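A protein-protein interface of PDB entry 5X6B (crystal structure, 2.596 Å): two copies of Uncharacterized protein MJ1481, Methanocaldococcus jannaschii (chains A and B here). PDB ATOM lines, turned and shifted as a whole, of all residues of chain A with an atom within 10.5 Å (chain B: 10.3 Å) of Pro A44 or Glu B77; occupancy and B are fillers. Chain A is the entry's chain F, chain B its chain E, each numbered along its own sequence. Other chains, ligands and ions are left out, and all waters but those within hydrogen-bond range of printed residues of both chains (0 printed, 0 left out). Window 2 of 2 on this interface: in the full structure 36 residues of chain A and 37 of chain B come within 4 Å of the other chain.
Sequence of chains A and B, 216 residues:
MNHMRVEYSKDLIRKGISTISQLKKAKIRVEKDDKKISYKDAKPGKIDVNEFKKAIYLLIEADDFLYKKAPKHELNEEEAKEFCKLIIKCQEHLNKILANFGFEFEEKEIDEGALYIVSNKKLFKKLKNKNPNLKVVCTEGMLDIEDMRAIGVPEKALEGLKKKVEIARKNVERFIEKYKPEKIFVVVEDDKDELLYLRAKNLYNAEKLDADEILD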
ATOM      1  N   SER A  38     -24.765  30.766 -19.076  1.00  0.00           N
ATOM      2  CA  SER A  38     -23.631  30.732 -19.997  1.00  0.00           C
ATOM      3  C   SER A  38     -22.530  29.811 -19.480  1.00  0.00           C
ATOM      4  O   SER A  38     -22.240  29.789 -18.281  1.00  0.00           O
ATOM      5  CB  SER A  38     -23.077  32.139 -20.216  1.00  0.00           C
ATOM      6  OG  SER A  38     -22.016  32.125 -21.157  1.00  0.00           O
ATOM      7  N   TYR A  39     -21.916  29.053 -20.383  1.00  0.00           N
ATOM      8  CA  TYR A  39     -20.877  28.114 -19.983  1.00  0.00           C
ATOM      9  C   TYR A  39     -19.677  28.863 -19.431  1.00  0.00           C
ATOM     10  O   TYR A  39     -18.964  28.355 -18.569  1.00  0.00           O
ATOM     11  CB  TYR A  39     -20.458  27.223 -21.152  1.00  0.00           C
ATOM     12  CG  TYR A  39     -19.684  27.923 -22.245  1.00  0.00           C
ATOM     13  CD1 TYR A  39     -18.293  27.965 -22.223  1.00  0.00           C
ATOM     14  CD2 TYR A  39     -20.341  28.531 -23.308  1.00  0.00           C
ATOM     15  CE1 TYR A  39     -17.580  28.601 -23.226  1.00  0.00           C
ATOM     16  CE2 TYR A  39     -19.638  29.168 -24.316  1.00  0.00           C
ATOM     17  CZ  TYR A  39     -18.259  29.200 -24.269  1.00  0.00           C
ATOM     18  OH  TYR A  39     -17.556  29.830 -25.269  1.00  0.00           O
ATOM     19  N   LYS A  40     -19.470  30.083 -19.922  1.00  0.00           N
ATOM     20  CA  LYS A  40     -18.344  30.906 -19.490  1.00  0.00           C
ATOM     21  C   LYS A  40     -18.391  31.174 -17.989  1.00  0.00           C
ATOM     22  O   LYS A  40     -17.369  31.467 -17.371  1.00  0.00           O
ATOM     23  CB  LYS A  40     -18.319  32.222 -20.266  1.00  0.00           C
ATOM     24  CG  LYS A  40     -18.212  32.032 -21.772  1.00  0.00           C
ATOM     25  CD  LYS A  40     -18.360  33.350 -22.514  1.00  0.00           C
ATOM     26  CE  LYS A  40     -18.246  33.155 -24.019  1.00  0.00           C
ATOM     27  NZ  LYS A  40     -18.499  34.414 -24.778  1.00  0.00           N
ATOM     28  N   ASP A  41     -19.577  31.050 -17.403  1.00  0.00           N
ATOM     29  CA  ASP A  41     -19.744  31.286 -15.975  1.00  0.00           C
ATOM     30  C   ASP A  41     -19.439  30.037 -15.157  1.00  0.00           C
ATOM     31  O   ASP A  41     -19.530  30.058 -13.928  1.00  0.00           O
ATOM     32  CB  ASP A  41     -21.167  31.774 -15.678  1.00  0.00           C
ATOM     33  CG  ASP A  41     -21.496  33.085 -16.374  1.00  0.00           C
ATOM     34  OD1 ASP A  41     -20.581  33.920 -16.553  1.00  0.00           O
ATOM     35  OD2 ASP A  41     -22.671  33.277 -16.754  1.00  0.00           O
ATOM     36  N   ALA A  42     -19.081  28.949 -15.835  1.00  0.00           N
ATOM     37  CA  ALA A  42     -18.831  27.689 -15.140  1.00  0.00           C
ATOM     38  C   ALA A  42     -17.635  27.821 -14.213  1.00  0.00           C
ATOM     39  O   ALA A  42     -16.629  28.428 -14.560  1.00  0.00           O
ATOM     40  CB  ALA A  42     -18.613  26.548 -16.132  1.00  0.00           C
ATOM     41  N   LYS A  43     -17.748  27.240 -13.031  1.00  0.00           N
ATOM     42  CA  LYS A  43     -16.684  27.320 -12.050  1.00  0.00           C
ATOM     43  C   LYS A  43     -16.132  25.925 -11.759  1.00  0.00           C
ATOM     44  O   LYS A  43     -16.808  24.930 -12.002  1.00  0.00           O
ATOM     45  CB  LYS A  43     -17.203  27.998 -10.778  1.00  0.00           C
ATOM     46  CG  LYS A  43     -17.822  29.364 -11.058  1.00  0.00           C
ATOM     47  CD  LYS A  43     -18.273  30.067  -9.797  1.00  0.00           C
ATOM     48  CE  LYS A  43     -18.823  31.450 -10.116  1.00  0.00           C
ATOM     49  NZ  LYS A  43     -19.991  31.382 -11.041  1.00  0.00           N
ATOM     50  N   PRO A  44     -14.881  25.850 -11.279  1.00  0.00           N
ATOM     51  CA  PRO A  44     -14.302  24.576 -10.853  1.00  0.00           C
ATOM     52  C   PRO A  44     -15.259  23.759  -9.991  1.00  0.00           C
ATOM     53  O   PRO A  44     -15.890  24.309  -9.088  1.00  0.00           O
ATOM     54  CB  PRO A  44     -13.079  25.011 -10.045  1.00  0.00           C
ATOM     55  CG  PRO A  44     -12.644  26.265 -10.721  1.00  0.00           C
ATOM     56  CD  PRO A  44     -13.900  26.950 -11.195  1.00  0.00           C
ATOM     57  N   GLY A  45     -15.366  22.466 -10.286  1.00  0.00           N
ATOM     58  CA  GLY A  45     -16.213  21.567  -9.527  1.00  0.00           C
ATOM     59  C   GLY A  45     -16.053  20.120  -9.955  1.00  0.00           C
ATOM     60  O   GLY A  45     -15.306  19.815 -10.885  1.00  0.00           O
ATOM     61  N   LYS A  46     -16.763  19.229  -9.272  1.00  0.00           N
ATOM     62  CA  LYS A  46     -16.642  17.790  -9.487  1.00  0.00           C
ATOM     63  C   LYS A  46     -17.786  17.228 -10.338  1.00  0.00           C
ATOM     64  O   LYS A  46     -18.951  17.559 -10.111  1.00  0.00           O
ATOM     65  CB  LYS A  46     -16.593  17.082  -8.129  1.00  0.00           C
ATOM     66  CG  LYS A  46     -16.608  15.564  -8.171  1.00  0.00           C
ATOM     67  CD  LYS A  46     -16.640  15.012  -6.752  1.00  0.00           C
ATOM     68  CE  LYS A  46     -16.620  13.489  -6.728  1.00  0.00           C
ATOM     69  NZ  LYS A  46     -16.658  12.971  -5.326  1.00  0.00           N
ATOM     70  N   ILE A  47     -17.459  16.383 -11.315  1.00  0.00           N
ATOM     71  CA  ILE A  47     -18.489  15.678 -12.082  1.00  0.00           C
ATOM     72  C   ILE A  47     -19.103  14.542 -11.278  1.00  0.00           C
ATOM     73  O   ILE A  47     -18.393  13.639 -10.841  1.00  0.00           O
ATOM     74  CB  ILE A  47     -17.958  15.053 -13.374  1.00  0.00           C
ATOM     75  CG1 ILE A  47     -17.319  16.095 -14.284  1.00  0.00           C
ATOM     76  CG2 ILE A  47     -19.100  14.366 -14.109  1.00  0.00           C
ATOM     77  CD1 ILE A  47     -16.752  15.482 -15.548  1.00  0.00           C
ATOM     78  N   ILE A  97     -25.900  18.056 -12.365  1.00  0.00           N
ATOM     79  CA  ILE A  97     -24.493  18.079 -12.737  1.00  0.00           C
ATOM     80  C   ILE A  97     -23.979  19.516 -12.838  1.00  0.00           C
ATOM     81  O   ILE A  97     -22.917  19.842 -12.309  1.00  0.00           O
ATOM     82  CB  ILE A  97     -24.260  17.350 -14.071  1.00  0.00           C
ATOM     83  CG1 ILE A  97     -24.688  15.885 -13.955  1.00  0.00           C
ATOM     84  CG2 ILE A  97     -22.800  17.445 -14.496  1.00  0.00           C
ATOM     85  CD1 ILE A  97     -24.635  15.139 -15.268  1.00  0.00           C
ATOM     86  N   LEU A  98     -24.749  20.371 -13.507  1.00  0.00           N
ATOM     87  CA  LEU A  98     -24.398  21.781 -13.667  1.00  0.00           C
ATOM     88  C   LEU A  98     -24.371  22.531 -12.335  1.00  0.00           C
ATOM     89  O   LEU A  98     -23.703  23.554 -12.206  1.00  0.00           O
ATOM     90  CB  LEU A  98     -25.377  22.472 -14.623  1.00  0.00           C
ATOM     91  CG  LEU A  98     -25.260  22.157 -16.116  1.00  0.00           C
ATOM     92  CD1 LEU A  98     -26.341  22.878 -16.905  1.00  0.00           C
ATOM     93  CD2 LEU A  98     -23.882  22.516 -16.647  1.00  0.00           C
ATOM     94  N   ALA A  99     -25.101  22.020 -11.350  1.00  0.00           N
ATOM     95  CA  ALA A  99     -25.148  22.652 -10.038  1.00  0.00           C
ATOM     96  C   ALA A  99     -23.793  22.558  -9.354  1.00  0.00           C
ATOM     97  O   ALA A  99     -23.451  23.394  -8.519  1.00  0.00           O
ATOM     98  CB  ALA A  99     -26.224  22.018  -9.176  1.00  0.00           C
ATOM     99  N   ASN A 100     -23.021  21.540  -9.722  1.00  0.00           N
ATOM    100  CA  ASN A 100     -21.696  21.338  -9.153  1.00  0.00           C
ATOM    101  C   ASN A 100     -20.656  22.283  -9.733  1.00  0.00           C
ATOM    102  O   ASN A 100     -19.515  22.317  -9.279  1.00  0.00           O
ATOM    103  CB  ASN A 100     -21.253  19.892  -9.353  1.00  0.00           C
ATOM    104  CG  ASN A 100     -21.897  18.955  -8.364  1.00  0.00           C
ATOM    105  OD1 ASN A 100     -22.240  19.359  -7.258  1.00  0.00           O
ATOM    106  ND2 ASN A 100     -22.069  17.696  -8.753  1.00  0.00           N
ATOM    107  N   PHE A 101     -21.052  23.056 -10.734  1.00  0.00           N
ATOM    108  CA  PHE A 101     -20.145  24.021 -11.335  1.00  0.00           C
ATOM    109  C   PHE A 101     -20.670  25.445 -11.204  1.00  0.00           C
ATOM    110  O   PHE A 101     -20.494  26.264 -12.104  1.00  0.00           O
ATOM    111  CB  PHE A 101     -19.903  23.667 -12.799  1.00  0.00           C
ATOM    112  CG  PHE A 101     -19.338  22.293 -12.992  1.00  0.00           C
ATOM    113  CD1 PHE A 101     -17.987  22.056 -12.805  1.00  0.00           C
ATOM    114  CD2 PHE A 101     -20.158  21.232 -13.340  1.00  0.00           C
ATOM    115  CE1 PHE A 101     -17.463  20.791 -12.973  1.00  0.00           C
ATOM    116  CE2 PHE A 101     -19.638  19.965 -13.509  1.00  0.00           C
ATOM    117  CZ  PHE A 101     -18.291  19.744 -13.322  1.00  0.00           C
ATOM    118  N   GLY A 102     -21.324  25.731 -10.082  1.00  0.00           N
ATOM    119  CA  GLY A 102     -21.721  27.086  -9.753  1.00  0.00           C
ATOM    120  C   GLY A 102     -23.114  27.484 -10.207  1.00  0.00           C
ATOM    121  O   GLY A 102     -23.690  28.444  -9.699  1.00  0.00           O
ATOM    122  N   PHE A 103     -23.658  26.754 -11.170  1.00  0.00           N
ATOM    123  CA  PHE A 103     -24.988  27.056 -11.678  1.00  0.00           C
ATOM    124  C   PHE A 103     -26.048  26.693 -10.642  1.00  0.00           C
ATOM    125  O   PHE A 103     -25.873  25.764  -9.856  1.00  0.00           O
ATOM    126  CB  PHE A 103     -25.238  26.318 -12.991  1.00  0.00           C
ATOM    127  CG  PHE A 103     -24.299  26.713 -14.090  1.00  0.00           C
ATOM    128  CD1 PHE A 103     -24.501  27.886 -14.800  1.00  0.00           C
ATOM    129  CD2 PHE A 103     -23.213  25.910 -14.417  1.00  0.00           C
ATOM    130  CE1 PHE A 103     -23.639  28.262 -15.819  1.00  0.00           C
ATOM    131  CE2 PHE A 103     -22.344  26.276 -15.439  1.00  0.00           C
ATOM    132  CZ  PHE A 103     -22.557  27.452 -16.141  1.00  0.00           C
ATOM    133  N   PHE B  65     -14.541  13.238 -20.412  1.00  0.00           N
ATOM    134  CA  PHE B  65     -14.095  13.786 -19.133  1.00  0.00           C
ATOM    135  C   PHE B  65     -14.176  12.749 -18.018  1.00  0.00           C
ATOM    136  O   PHE B  65     -13.379  12.773 -17.082  1.00  0.00           O
ATOM    137  CB  PHE B  65     -14.912  15.028 -18.758  1.00  0.00           C
ATOM    138  CG  PHE B  65     -14.533  16.266 -19.531  1.00  0.00           C
ATOM    139  CD1 PHE B  65     -13.798  17.276 -18.929  1.00  0.00           C
ATOM    140  CD2 PHE B  65     -14.909  16.417 -20.857  1.00  0.00           C
ATOM    141  CE1 PHE B  65     -13.450  18.414 -19.630  1.00  0.00           C
ATOM    142  CE2 PHE B  65     -14.565  17.553 -21.569  1.00  0.00           C
ATOM    143  CZ  PHE B  65     -13.832  18.552 -20.954  1.00  0.00           C
ATOM    144  N   LYS B  69     -10.485  12.304 -16.435  1.00  0.00           N
ATOM    145  CA  LYS B  69     -10.401  12.941 -15.127  1.00  0.00           C
ATOM    146  C   LYS B  69     -10.613  11.935 -14.006  1.00  0.00           C
ATOM    147  O   LYS B  69     -10.640  12.292 -12.826  1.00  0.00           O
ATOM    148  CB  LYS B  69     -11.411  14.088 -15.022  1.00  0.00           C
ATOM    149  CG  LYS B  69     -11.343  15.081 -16.179  1.00  0.00           C
ATOM    150  CD  LYS B  69      -9.953  15.689 -16.330  1.00  0.00           C
ATOM    151  CE  LYS B  69      -9.508  16.414 -15.064  1.00  0.00           C
ATOM    152  NZ  LYS B  69      -8.143  16.998 -15.221  1.00  0.00           N
ATOM    153  N   HIS B  73     -12.382  12.974 -10.791  1.00  0.00           N
ATOM    154  CA  HIS B  73     -13.224  13.788 -11.669  1.00  0.00           C
ATOM    155  C   HIS B  73     -13.402  15.226 -11.190  1.00  0.00           C
ATOM    156  O   HIS B  73     -14.493  15.786 -11.274  1.00  0.00           O
ATOM    157  CB  HIS B  73     -14.598  13.138 -11.834  1.00  0.00           C
ATOM    158  CG  HIS B  73     -14.541  11.763 -12.424  1.00  0.00           C
ATOM    159  ND1 HIS B  73     -14.725  10.627 -11.666  1.00  0.00           N
ATOM    160  CD2 HIS B  73     -14.305  11.344 -13.685  1.00  0.00           C
ATOM    161  CE1 HIS B  73     -14.611   9.563 -12.442  1.00  0.00           C
ATOM    162  NE2 HIS B  73     -14.356   9.971 -13.674  1.00  0.00           N
ATOM    163  N   GLU B  74     -12.328  15.813 -10.678  1.00  0.00           N
ATOM    164  CA  GLU B  74     -12.356  17.211 -10.274  1.00  0.00           C
ATOM    165  C   GLU B  74     -11.867  18.082 -11.421  1.00  0.00           C
ATOM    166  O   GLU B  74     -10.747  17.917 -11.905  1.00  0.00           O
ATOM    167  CB  GLU B  74     -11.517  17.416  -9.014  1.00  0.00           C
ATOM    168  CG  GLU B  74     -12.100  16.705  -7.790  1.00  0.00           C
ATOM    169  CD  GLU B  74     -11.156  16.687  -6.602  1.00  0.00           C
ATOM    170  OE1 GLU B  74     -10.003  17.143  -6.749  1.00  0.00           O
ATOM    171  OE2 GLU B  74     -11.565  16.203  -5.524  1.00  0.00           O
ATOM    172  N   LEU B  75     -12.720  18.995 -11.875  1.00  0.00           N
ATOM    173  CA  LEU B  75     -12.392  19.837 -13.021  1.00  0.00           C
ATOM    174  C   LEU B  75     -11.860  21.189 -12.576  1.00  0.00           C
ATOM    175  O   LEU B  75     -12.218  21.688 -11.506  1.00  0.00           O
ATOM    176  CB  LEU B  75     -13.616  20.033 -13.921  1.00  0.00           C
ATOM    177  CG  LEU B  75     -14.286  18.776 -14.478  1.00  0.00           C
ATOM    178  CD1 LEU B  75     -15.413  19.142 -15.431  1.00  0.00           C
ATOM    179  CD2 LEU B  75     -13.263  17.884 -15.168  1.00  0.00           C
ATOM    180  N   ASN B  76     -10.993  21.779 -13.393  1.00  0.00           N
ATOM    181  CA  ASN B  76     -10.547  23.137 -13.135  1.00  0.00           C
ATOM    182  C   ASN B  76     -11.412  24.091 -13.948  1.00  0.00           C
ATOM    183  O   ASN B  76     -12.327  23.651 -14.637  1.00  0.00           O
ATOM    184  CB  ASN B  76      -9.061  23.308 -13.458  1.00  0.00           C
ATOM    185  CG  ASN B  76      -8.725  22.990 -14.896  1.00  0.00           C
ATOM    186  OD1 ASN B  76      -9.507  23.246 -15.813  1.00  0.00           O
ATOM    187  ND2 ASN B  76      -7.532  22.453 -15.105  1.00  0.00           N
ATOM    188  N   GLU B  77     -11.117  25.383 -13.884  1.00  0.00           N
ATOM    189  CA  GLU B  77     -11.979  26.382 -14.503  1.00  0.00           C
ATOM    190  C   GLU B  77     -12.072  26.215 -16.023  1.00  0.00           C
ATOM    191  O   GLU B  77     -13.152  26.347 -16.597  1.00  0.00           O
ATOM    192  CB  GLU B  77     -11.492  27.789 -14.146  1.00  0.00           C
ATOM    193  CG  GLU B  77     -12.456  28.902 -14.520  1.00  0.00           C
ATOM    194  CD  GLU B  77     -12.120  29.540 -15.847  1.00  0.00           C
ATOM    195  OE1 GLU B  77     -11.023  29.257 -16.378  1.00  0.00           O
ATOM    196  OE2 GLU B  77     -12.945  30.332 -16.351  1.00  0.00           O
ATOM    197  N   GLU B  78     -10.948  25.916 -16.669  1.00  0.00           N
ATOM    198  CA  GLU B  78     -10.940  25.697 -18.118  1.00  0.00           C
ATOM    199  C   GLU B  78     -11.725  24.435 -18.482  1.00  0.00           C
ATOM    200  O   GLU B  78     -12.559  24.442 -19.394  1.00  0.00           O
ATOM    201  CB  GLU B  78      -9.507  25.592 -18.646  1.00  0.00           C
ATOM    202  CG  GLU B  78      -9.397  25.499 -20.162  1.00  0.00           C
ATOM    203  CD  GLU B  78      -7.967  25.264 -20.636  1.00  0.00           C
ATOM    204  OE1 GLU B  78      -7.055  25.185 -19.786  1.00  0.00           O
ATOM    205  OE2 GLU B  78      -7.758  25.151 -21.863  1.00  0.00           O
ATOM    206  N   GLU B  79     -11.450  23.353 -17.757  1.00  0.00           N
ATOM    207  CA  GLU B  79     -12.149  22.091 -17.967  1.00  0.00           C
ATOM    208  C   GLU B  79     -13.641  22.211 -17.669  1.00  0.00           C
ATOM    209  O   GLU B  79     -14.464  21.607 -18.358  1.00  0.00           O
ATOM    210  CB  GLU B  79     -11.530  20.988 -17.106  1.00  0.00           C
ATOM    211  CG  GLU B  79     -10.149  20.550 -17.561  1.00  0.00           C
ATOM    212  CD  GLU B  79      -9.404  19.769 -16.496  1.00  0.00           C
ATOM    213  OE1 GLU B  79      -9.782  19.871 -15.310  1.00  0.00           O
ATOM    214  OE2 GLU B  79      -8.442  19.051 -16.841  1.00  0.00           O
ATOM    215  N   ALA B  80     -13.981  22.993 -16.649  1.00  0.00           N
ATOM    216  CA  ALA B  80     -15.376  23.195 -16.274  1.00  0.00           C
ATOM    217  C   ALA B  80     -16.152  23.875 -17.395  1.00  0.00           C
ATOM    218  O   ALA B  80     -17.244  23.439 -17.753  1.00  0.00           O
ATOM    219  CB  ALA B  80     -15.478  24.003 -15.000  1.00  0.00           C
ATOM    220  N   LYS B  81     -15.581  24.934 -17.959  1.00  0.00           N
ATOM    221  CA  LYS B  81     -16.232  25.641 -19.054  1.00  0.00           C
ATOM    222  C   LYS B  81     -16.385  24.760 -20.289  1.00  0.00           C
ATOM    223  O   LYS B  81     -17.410  24.805 -20.966  1.00  0.00           O
ATOM    224  CB  LYS B  81     -15.459  26.910 -19.413  1.00  0.00           C
ATOM    225  CG  LYS B  81     -15.561  28.008 -18.370  1.00  0.00           C
ATOM    226  CD  LYS B  81     -15.012  29.314 -18.905  1.00  0.00           C
ATOM    227  CE  LYS B  81     -13.562  29.178 -19.321  1.00  0.00           C
ATOM    228  NZ  LYS B  81     -13.056  30.428 -19.950  1.00  0.00           N
ATOM    229  N   GLU B  82     -15.368  23.959 -20.581  1.00  0.00           N
ATOM    230  CA  GLU B  82     -15.397  23.098 -21.760  1.00  0.00           C
ATOM    231  C   GLU B  82     -16.470  22.025 -21.598  1.00  0.00           C
ATOM    232  O   GLU B  82     -17.231  21.729 -22.525  1.00  0.00           O
ATOM    233  CB  GLU B  82     -14.022  22.465 -21.981  1.00  0.00           C
ATOM    234  CG  GLU B  82     -13.890  21.627 -23.239  1.00  0.00           C
ATOM    235  CD  GLU B  82     -12.505  21.019 -23.380  1.00  0.00           C
ATOM    236  OE1 GLU B  82     -11.659  21.254 -22.488  1.00  0.00           O
ATOM    237  OE2 GLU B  82     -12.264  20.303 -24.378  1.00  0.00           O
ATOM    238  N   PHE B  83     -16.533  21.467 -20.395  1.00  0.00           N
ATOM    239  CA  PHE B  83     -17.468  20.405 -20.074  1.00  0.00           C
ATOM    240  C   PHE B  83     -18.911  20.890 -20.009  1.00  0.00           C
ATOM    241  O   PHE B  83     -19.802  20.293 -20.619  1.00  0.00           O
ATOM    242  CB  PHE B  83     -17.087  19.765 -18.741  1.00  0.00           C
ATOM    243  CG  PHE B  83     -18.032  18.694 -18.295  1.00  0.00           C
ATOM    244  CD1 PHE B  83     -18.047  17.463 -18.930  1.00  0.00           C
ATOM    245  CD2 PHE B  83     -18.902  18.915 -17.237  1.00  0.00           C
ATOM    246  CE1 PHE B  83     -18.914  16.465 -18.519  1.00  0.00           C
ATOM    247  CE2 PHE B  83     -19.770  17.923 -16.814  1.00  0.00           C
ATOM    248  CZ  PHE B  83     -19.775  16.692 -17.457  1.00  0.00           C
ATOM    249  N   CYS B  84     -19.142  21.963 -19.260  1.00  0.00           N
ATOM    250  CA  CYS B  84     -20.497  22.473 -19.072  1.00  0.00           C
ATOM    251  C   CYS B  84     -21.037  23.029 -20.387  1.00  0.00           C
ATOM    252  O   CYS B  84     -22.245  23.020 -20.619  1.00  0.00           O
ATOM    253  CB  CYS B  84     -20.543  23.540 -17.963  1.00  0.00           C
ATOM    254  SG  CYS B  84     -20.191  22.936 -16.303  1.00  0.00           S
ATOM    255  N   LYS B  85     -20.144  23.494 -21.252  1.00  0.00           N
ATOM    256  CA  LYS B  85     -20.554  23.941 -22.577  1.00  0.00           C
ATOM    257  C   LYS B  85     -21.269  22.816 -23.314  1.00  0.00           C
ATOM    258  O   LYS B  85     -22.300  23.036 -23.952  1.00  0.00           O
ATOM    259  CB  LYS B  85     -19.354  24.426 -23.388  1.00  0.00           C
ATOM    260  CG  LYS B  85     -19.728  25.059 -24.717  1.00  0.00           C
ATOM    261  CD  LYS B  85     -18.502  25.341 -25.561  1.00  0.00           C
ATOM    262  CE  LYS B  85     -18.878  26.020 -26.869  1.00  0.00           C
ATOM    263  NZ  LYS B  85     -17.718  26.092 -27.808  1.00  0.00           N
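Of the 15 printed residues of chain B, 10 touch a printed residue of chain A.
Hydrophobic or aromatic side chains of chain B within 4 Å of the printed part of chain A: Phe B65, His B73, Leu B75, Ala B80 and Phe B83.
Of the 17 printed residues of chain A, 11 touch a printed residue of chain B.
Printed residues of chain A that touch a printed residue of chain B: Tyr A39, Lys A40, Ala A42, Lys A43, Pro A44, Gly A45, Lys A46, Ile A47, Ile A97, Leu A98 and Phe A101.
Hydrophobic or aromatic side chains of chain A within 4 Å of the printed part of chain B: Tyr A39, Ala A42, Pro A44, Ile A47, Ile A97, Leu A98 and Phe A101.
Among the printed residues, 22 pairs touch across the chains.
Among the printed residues, no Asp or Glu carboxylate lies within 4 Å of a Lys or Arg side-chain nitrogen of the other chain.
No position is printed for both chains.
Of the 22 pairs that touch across the chains among the printed residues, none has its exchanged pair printed and touching as well.
NZ of Lys B81 lies within salt-bridge range of OE2 of Glu B77 (3.6 Å).
The side-chain sulfur of Cys B84 lies close to the backbone carbonyl oxygen of Ala B80, 3.3 Å away.
O of Asp A41 lies within hydrogen-bond range of NZ of Lys A43, at 3.2 Å.
The backbone NH (N) of Lys A43 sits at hydrogen-bond distance from the backbone carbonyl oxygen (O) of Phe A101 (3.1 Å).
The backbone carbonyl oxygen (O) of Lys A46 lies close to the side-chain amide nitrogen (ND2) of Asn A100 (3.4 Å).
The backbone carbonyl oxygen (O) of Leu A98 lies close to the backbone NH (N) of Phe A103, 3.4 Å away.
Among the printed residues, pairs that only touch across the chains: Tyr A39 with Lys B81 (3.4 Å), Tyr A39 with Lys B85 (3.6 Å), Lys A40 with Lys B81 (3.5 Å), Ala A42 with Ala B80 (3.8 Å), Ala A42 with Lys B81 (3.9 Å), Ala A42 with Cys B84 (3.9 Å), Lys A43 with Ala B80 (3.4 Å), Pro A44 with Leu B75 (3.6 Å), Pro A44 with Glu B77 (3.6 Å), Gly A45 with Glu B74 (3.9 Å), Lys A46 with His B73 (3.4 Å), Ile A47 with Phe B65 (3.7 Å), Ile A47 with Leu B75 (3.8 Å), Ile A47 with Phe B83 (3.8 Å), Ile A97 with Phe B83 (3.8 Å), Leu A98 with Cys B84 (3.7 Å), Phe A101 with Leu B75 (3.6 Å), Phe A101 with Ala B80 (3.9 Å), Phe A101 with Phe B83 (3.9 Å) and Phe A101 with Cys B84 (3.4 Å).
Of chain B, only Glu B74 (3.9 Å) and Leu B75 (2.9 Å) come within 4 Å of Gly A45.
No residue of chain A comes within 4 Å of Asn B76.
Of chain A, only Ala A42 (3.8 Å), Lys A43 (3.4 Å) and Phe A101 (3.9 Å) come within 4 Å of Ala B80.
Lys B81 touches three residues of chain A.
Of the printed residues of chain B, Lys A43 touches Ala B80.
Of the printed residues of chain B, Phe A101 touches Leu B75, Ala B80, Phe B83 and Cys B84.
Printed residues of chain B within 4 Å of Lys A46: His B73 (3.4 Å).
Printed residues of chain A within 4 Å of Phe B83: Ile A47 (3.8 Å), Ile A97 (3.8 Å) and Phe A101 (3.9 Å).
Asn A100 touches none of the printed residues of chain B.
Phe A103 touches none of the printed residues of chain B.
The nearest residue of chain B that does not touch Pro A44 is Asn B76 (4.1 Å).
The nearest residue of chain A that does not touch Glu B77 is Ala A42 (4.2 Å).
The nearest printed residue of chain B that does not touch Lys A46 is Glu B74 (4.4 Å).
The backbone NH of Ile A47 sits at hydrogen-bond distance from the backbone carbonyl oxygen of His B73 (3.0 Å).
N of Leu B75 lies within hydrogen-bond range of O of Gly A45 (2.9 Å).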
